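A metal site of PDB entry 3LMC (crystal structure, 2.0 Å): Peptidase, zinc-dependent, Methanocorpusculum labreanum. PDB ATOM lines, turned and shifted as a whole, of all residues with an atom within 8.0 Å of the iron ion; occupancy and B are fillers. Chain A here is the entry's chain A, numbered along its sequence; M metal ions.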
ATOM      1  N   LEU A 157     -25.759  13.409 -25.774  1.00  0.00           N
ATOM      2  CA  LEU A 157     -24.495  12.736 -25.465  1.00  0.00           C
ATOM      3  C   LEU A 157     -24.732  11.339 -24.919  1.00  0.00           C
ATOM      4  O   LEU A 157     -25.668  11.102 -24.147  1.00  0.00           O
ATOM      5  CB  LEU A 157     -23.668  13.551 -24.482  1.00  0.00           C
ATOM      6  CG  LEU A 157     -22.911  14.769 -25.012  1.00  0.00           C
ATOM      7  CD1 LEU A 157     -23.902  15.839 -25.434  1.00  0.00           C
ATOM      8  CD2 LEU A 157     -21.975  15.291 -23.946  1.00  0.00           C
ATOM      9  N   GLY A 158     -23.873  10.397 -25.317  1.00  0.00           N
ATOM     10  CA  GLY A 158     -23.931   9.059 -24.763  1.00  0.00           C
ATOM     11  C   GLY A 158     -22.897   8.906 -23.671  1.00  0.00           C
ATOM     12  O   GLY A 158     -22.321   9.896 -23.219  1.00  0.00           O
ATOM     13  N   HIS A 159     -22.635   7.679 -23.244  1.00  0.00           N
ATOM     14  CA  HIS A 159     -21.610   7.455 -22.225  1.00  0.00           C
ATOM     15  C   HIS A 159     -20.197   7.585 -22.749  1.00  0.00           C
ATOM     16  O   HIS A 159     -19.880   7.110 -23.832  1.00  0.00           O
ATOM     17  CB  HIS A 159     -21.783   6.091 -21.567  1.00  0.00           C
ATOM     18  CG  HIS A 159     -22.954   6.028 -20.637  1.00  0.00           C
ATOM     19  ND1 HIS A 159     -23.763   4.915 -20.536  1.00  0.00           N
ATOM     20  CD2 HIS A 159     -23.461   6.950 -19.804  1.00  0.00           C
ATOM     21  CE1 HIS A 159     -24.714   5.158 -19.654  1.00  0.00           C
ATOM     22  NE2 HIS A 159     -24.550   6.390 -19.188  1.00  0.00           N
ATOM     23  N   CYS A 160     -19.358   8.224 -21.949  1.00  0.00           N
ATOM     24  CA  CYS A 160     -17.991   8.489 -22.342  1.00  0.00           C
ATOM     25  C   CYS A 160     -17.051   7.492 -21.672  1.00  0.00           C
ATOM     26  O   CYS A 160     -17.336   6.999 -20.567  1.00  0.00           O
ATOM     27  CB  CYS A 160     -17.658   9.915 -21.913  1.00  0.00           C
ATOM     28  SG  CYS A 160     -16.009  10.427 -22.267  1.00  0.00           S
ATOM     29  N   ASP A 161     -15.943   7.197 -22.351  1.00  0.00           N
ATOM     30  CA  ASP A 161     -14.940   6.249 -21.874  1.00  0.00           C
ATOM     31  C   ASP A 161     -13.960   6.812 -20.840  1.00  0.00           C
ATOM     32  O   ASP A 161     -13.331   6.066 -20.092  1.00  0.00           O
ATOM     33  CB  ASP A 161     -14.130   5.700 -23.050  1.00  0.00           C
ATOM     34  CG  ASP A 161     -14.806   4.545 -23.728  1.00  0.00           C
ATOM     35  OD1 ASP A 161     -15.697   3.934 -23.072  1.00  0.00           O
ATOM     36  OD2 ASP A 161     -14.467   4.255 -24.888  1.00  0.00           O
ATOM     37  N   ASN A 162     -13.825   8.136 -20.849  1.00  0.00           N
ATOM     38  CA  ASN A 162     -12.935   8.857 -19.936  1.00  0.00           C
ATOM     39  C   ASN A 162     -13.557   8.940 -18.536  1.00  0.00           C
ATOM     40  O   ASN A 162     -14.532   9.656 -18.334  1.00  0.00           O
ATOM     41  CB  ASN A 162     -12.663  10.247 -20.517  1.00  0.00           C
ATOM     42  CG  ASN A 162     -11.688  11.039 -19.688  1.00  0.00           C
ATOM     43  OD1 ASN A 162     -11.413  10.706 -18.529  1.00  0.00           O
ATOM     44  ND2 ASN A 162     -11.140  12.107 -20.276  1.00  0.00           N
ATOM     45  N   PRO A 163     -12.980   8.211 -17.566  1.00  0.00           N
ATOM     46  CA  PRO A 163     -13.499   8.033 -16.189  1.00  0.00           C
ATOM     47  C   PRO A 163     -13.515   9.331 -15.365  1.00  0.00           C
ATOM     48  O   PRO A 163     -14.174   9.398 -14.315  1.00  0.00           O
ATOM     49  CB  PRO A 163     -12.504   7.033 -15.561  1.00  0.00           C
ATOM     50  CG  PRO A 163     -11.768   6.417 -16.723  1.00  0.00           C
ATOM     51  CD  PRO A 163     -11.716   7.491 -17.778  1.00  0.00           C
ATOM     52  N   GLY A 164     -12.774  10.343 -15.822  1.00  0.00           N
ATOM     53  CA  GLY A 164     -12.828  11.661 -15.230  1.00  0.00           C
ATOM     54  C   GLY A 164     -13.886  12.559 -15.847  1.00  0.00           C
ATOM     55  O   GLY A 164     -14.160  13.639 -15.331  1.00  0.00           O
ATOM     56  N   CYS A 165     -14.494  12.132 -16.951  1.00  0.00           N
ATOM     57  CA  CYS A 165     -15.502  12.958 -17.618  1.00  0.00           C
ATOM     58  C   CYS A 165     -16.891  12.777 -17.023  1.00  0.00           C
ATOM     59  O   CYS A 165     -17.250  11.681 -16.559  1.00  0.00           O
ATOM     60  CB  CYS A 165     -15.547  12.659 -19.126  1.00  0.00           C
ATOM     61  SG  CYS A 165     -16.833  13.617 -20.000  1.00  0.00           S
ATOM     62  N   ILE A 166     -17.682  13.842 -17.031  1.00  0.00           N
ATOM     63  CA  ILE A 166     -19.024  13.838 -16.466  1.00  0.00           C
ATOM     64  C   ILE A 166     -19.903  12.756 -17.099  1.00  0.00           C
ATOM     65  O   ILE A 166     -20.799  12.205 -16.438  1.00  0.00           O
ATOM     66  CB  ILE A 166     -19.726  15.194 -16.666  1.00  0.00           C
ATOM     67  CG1 ILE A 166     -19.114  16.245 -15.741  1.00  0.00           C
ATOM     68  CG2 ILE A 166     -21.228  15.065 -16.388  1.00  0.00           C
ATOM     69  CD1 ILE A 166     -19.823  16.415 -14.448  1.00  0.00           C
ATOM     70  N   MET A 167     -19.628  12.441 -18.365  1.00  0.00           N
ATOM     71  CA  MET A 167     -20.447  11.497 -19.140  1.00  0.00           C
ATOM     72  C   MET A 167     -20.083  10.024 -18.924  1.00  0.00           C
ATOM     73  O   MET A 167     -20.728   9.133 -19.483  1.00  0.00           O
ATOM     74  CB  MET A 167     -20.400  11.805 -20.644  1.00  0.00           C
ATOM     75  CG  MET A 167     -21.160  13.031 -21.080  1.00  0.00           C
ATOM     76  SD  MET A 167     -22.915  13.276 -20.178  1.00  0.00           S
ATOM     77  CE  MET A 167     -23.190  15.110 -20.746  1.00  0.00           C
ATOM     78  N   TYR A 168     -19.056   9.766 -18.128  1.00  0.00           N
ATOM     79  CA  TYR A 168     -18.699   8.405 -17.777  1.00  0.00           C
ATOM     80  C   TYR A 168     -19.820   7.811 -16.919  1.00  0.00           C
ATOM     81  O   TYR A 168     -20.418   8.513 -16.105  1.00  0.00           O
ATOM     82  CB  TYR A 168     -17.397   8.407 -16.994  1.00  0.00           C
ATOM     83  CG  TYR A 168     -16.953   7.035 -16.535  1.00  0.00           C
ATOM     84  CD1 TYR A 168     -17.071   6.661 -15.201  1.00  0.00           C
ATOM     85  CD2 TYR A 168     -16.409   6.119 -17.421  1.00  0.00           C
ATOM     86  CE1 TYR A 168     -16.682   5.408 -14.775  1.00  0.00           C
ATOM     87  CE2 TYR A 168     -16.015   4.875 -17.005  1.00  0.00           C
ATOM     88  CZ  TYR A 168     -16.150   4.517 -15.679  1.00  0.00           C
ATOM     89  OH  TYR A 168     -15.753   3.275 -15.249  1.00  0.00           O
ATOM     90  N   TYR A 182     -16.256  18.172 -15.082  1.00  0.00           N
ATOM     91  CA  TYR A 182     -15.436  18.214 -16.291  1.00  0.00           C
ATOM     92  C   TYR A 182     -16.118  17.487 -17.440  1.00  0.00           C
ATOM     93  O   TYR A 182     -16.498  16.330 -17.314  1.00  0.00           O
ATOM     94  CB  TYR A 182     -14.097  17.514 -15.972  1.00  0.00           C
ATOM     95  CG  TYR A 182     -13.125  17.321 -17.118  1.00  0.00           C
ATOM     96  CD1 TYR A 182     -12.492  18.403 -17.697  1.00  0.00           C
ATOM     97  CD2 TYR A 182     -12.815  16.049 -17.591  1.00  0.00           C
ATOM     98  CE1 TYR A 182     -11.587  18.246 -18.733  1.00  0.00           C
ATOM     99  CE2 TYR A 182     -11.900  15.879 -18.642  1.00  0.00           C
ATOM    100  CZ  TYR A 182     -11.300  16.981 -19.203  1.00  0.00           C
ATOM    101  OH  TYR A 182     -10.387  16.835 -20.235  1.00  0.00           O
ATOM    102  N   PHE A 183     -16.305  18.176 -18.561  1.00  0.00           N
ATOM    103  CA  PHE A 183     -16.640  17.508 -19.796  1.00  0.00           C
ATOM    104  C   PHE A 183     -15.371  17.434 -20.633  1.00  0.00           C
ATOM    105  O   PHE A 183     -14.779  18.476 -20.930  1.00  0.00           O
ATOM    106  CB  PHE A 183     -17.690  18.300 -20.572  1.00  0.00           C
ATOM    107  CG  PHE A 183     -19.086  18.154 -20.041  1.00  0.00           C
ATOM    108  CD1 PHE A 183     -19.849  17.062 -20.381  1.00  0.00           C
ATOM    109  CD2 PHE A 183     -19.641  19.118 -19.220  1.00  0.00           C
ATOM    110  CE1 PHE A 183     -21.123  16.928 -19.901  1.00  0.00           C
ATOM    111  CE2 PHE A 183     -20.923  18.981 -18.738  1.00  0.00           C
ATOM    112  CZ  PHE A 183     -21.668  17.887 -19.089  1.00  0.00           C
ATOM    113  N   CYS A 184     -14.963  16.233 -21.023  1.00  0.00           N
ATOM    114  CA  CYS A 184     -13.754  16.089 -21.841  1.00  0.00           C
ATOM    115  C   CYS A 184     -13.910  16.783 -23.197  1.00  0.00           C
ATOM    116  O   CYS A 184     -14.984  17.331 -23.502  1.00  0.00           O
ATOM    117  CB  CYS A 184     -13.388  14.620 -22.045  1.00  0.00           C
ATOM    118  SG  CYS A 184     -14.441  13.739 -23.216  1.00  0.00           S
ATOM    119  N   GLY A 185     -12.861  16.761 -23.996  1.00  0.00           N
ATOM    120  CA  GLY A 185     -12.859  17.471 -25.272  1.00  0.00           C
ATOM    121  C   GLY A 185     -13.926  16.957 -26.216  1.00  0.00           C
ATOM    122  O   GLY A 185     -14.700  17.728 -26.797  1.00  0.00           O
ATOM    123  N   LYS A 186     -13.951  15.633 -26.392  1.00  0.00           N
ATOM    124  CA  LYS A 186     -14.948  14.991 -27.223  1.00  0.00           C
ATOM    125  C   LYS A 186     -16.370  15.414 -26.803  1.00  0.00           C
ATOM    126  O   LYS A 186     -17.204  15.754 -27.635  1.00  0.00           O
ATOM    127  CB  LYS A 186     -14.794  13.478 -27.146  1.00  0.00           C
ATOM    128  CG  LYS A 186     -15.782  12.721 -28.023  1.00  0.00           C
ATOM    129  CD  LYS A 186     -15.698  11.218 -27.799  1.00  0.00           C
ATOM    130  CE  LYS A 186     -15.955  10.842 -26.347  1.00  0.00           C
ATOM    131  NZ  LYS A 186     -17.302  11.285 -25.910  1.00  0.00           N
ATOM    132  N   CYS A 187     -16.642  15.382 -25.508  1.00  0.00           N
ATOM    133  CA  CYS A 187     -17.992  15.686 -25.036  1.00  0.00           C
ATOM    134  C   CYS A 187     -18.356  17.160 -25.171  1.00  0.00           C
ATOM    135  O   CYS A 187     -19.482  17.463 -25.572  1.00  0.00           O
ATOM    136  CB  CYS A 187     -18.221  15.172 -23.630  1.00  0.00           C
ATOM    137  SG  CYS A 187     -18.203  13.375 -23.490  1.00  0.00           S
ATOM    138  N   ARG A 188     -17.440  18.081 -24.854  1.00  0.00           N
ATOM    139  CA  ARG A 188     -17.755  19.508 -25.020  1.00  0.00           C
ATOM    140  C   ARG A 188     -18.147  19.889 -26.472  1.00  0.00           C
ATOM    141  O   ARG A 188     -19.086  20.667 -26.666  1.00  0.00           O
ATOM    142  CB  ARG A 188     -16.661  20.450 -24.459  1.00  0.00           C
ATOM    143  CG  ARG A 188     -15.217  20.068 -24.715  1.00  0.00           C
ATOM    144  CD  ARG A 188     -14.277  20.821 -23.739  1.00  0.00           C
ATOM    145  NE  ARG A 188     -12.896  20.327 -23.754  1.00  0.00           N
ATOM    146  CZ  ARG A 188     -12.054  20.404 -22.723  1.00  0.00           C
ATOM    147  NH1 ARG A 188     -12.450  20.941 -21.583  1.00  0.00           N
ATOM    148  NH2 ARG A 188     -10.821  19.918 -22.833  1.00  0.00           N
ATOM    149  N   GLN A 190     -19.566  17.943 -28.789  1.00  0.00           N
ATOM    150  CA  GLN A 190     -20.915  17.437 -29.024  1.00  0.00           C
ATOM    151  C   GLN A 190     -21.961  18.280 -28.316  1.00  0.00           C
ATOM    152  O   GLN A 190     -23.024  18.584 -28.878  1.00  0.00           O
ATOM    153  CB  GLN A 190     -21.051  15.979 -28.570  1.00  0.00           C
ATOM    154  CG  GLN A 190     -20.120  15.029 -29.298  1.00  0.00           C
ATOM    155  CD  GLN A 190     -20.215  13.616 -28.766  1.00  0.00           C
ATOM    156  OE1 GLN A 190     -19.220  12.888 -28.748  1.00  0.00           O
ATOM    157  NE2 GLN A 190     -21.396  13.225 -28.302  1.00  0.00           N
HETATM  158 FE    FE M   1     -16.316  12.775 -22.205  1.00  0.00          FE
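O of Met 167 lies within hydrogen-bond range of N of Cys 160, at 3.0 Å.
N of Met 167 lies close to SG of Cys 165 (3.4 Å).
The backbone NH (N) of Lys 186 lies close to the side-chain sulfur (SG) of Cys 184.
The side-chain amino group (NZ) of Lys 186 lies close to the side-chain sulfur (SG) of Cys 187, 3.3 Å away.
SG of Cys 160 lies close to N of Asn 162 (3.5 Å).
The iron ion is bound by the side-chain sulfur (SG) of Cys 184, the side-chain sulfur (SG) of Cys 187, the side-chain sulfur (SG) of Cys 160 and the side-chain sulfur (SG) of Cys 165.
The iron ion has four donor atoms within binding distance.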
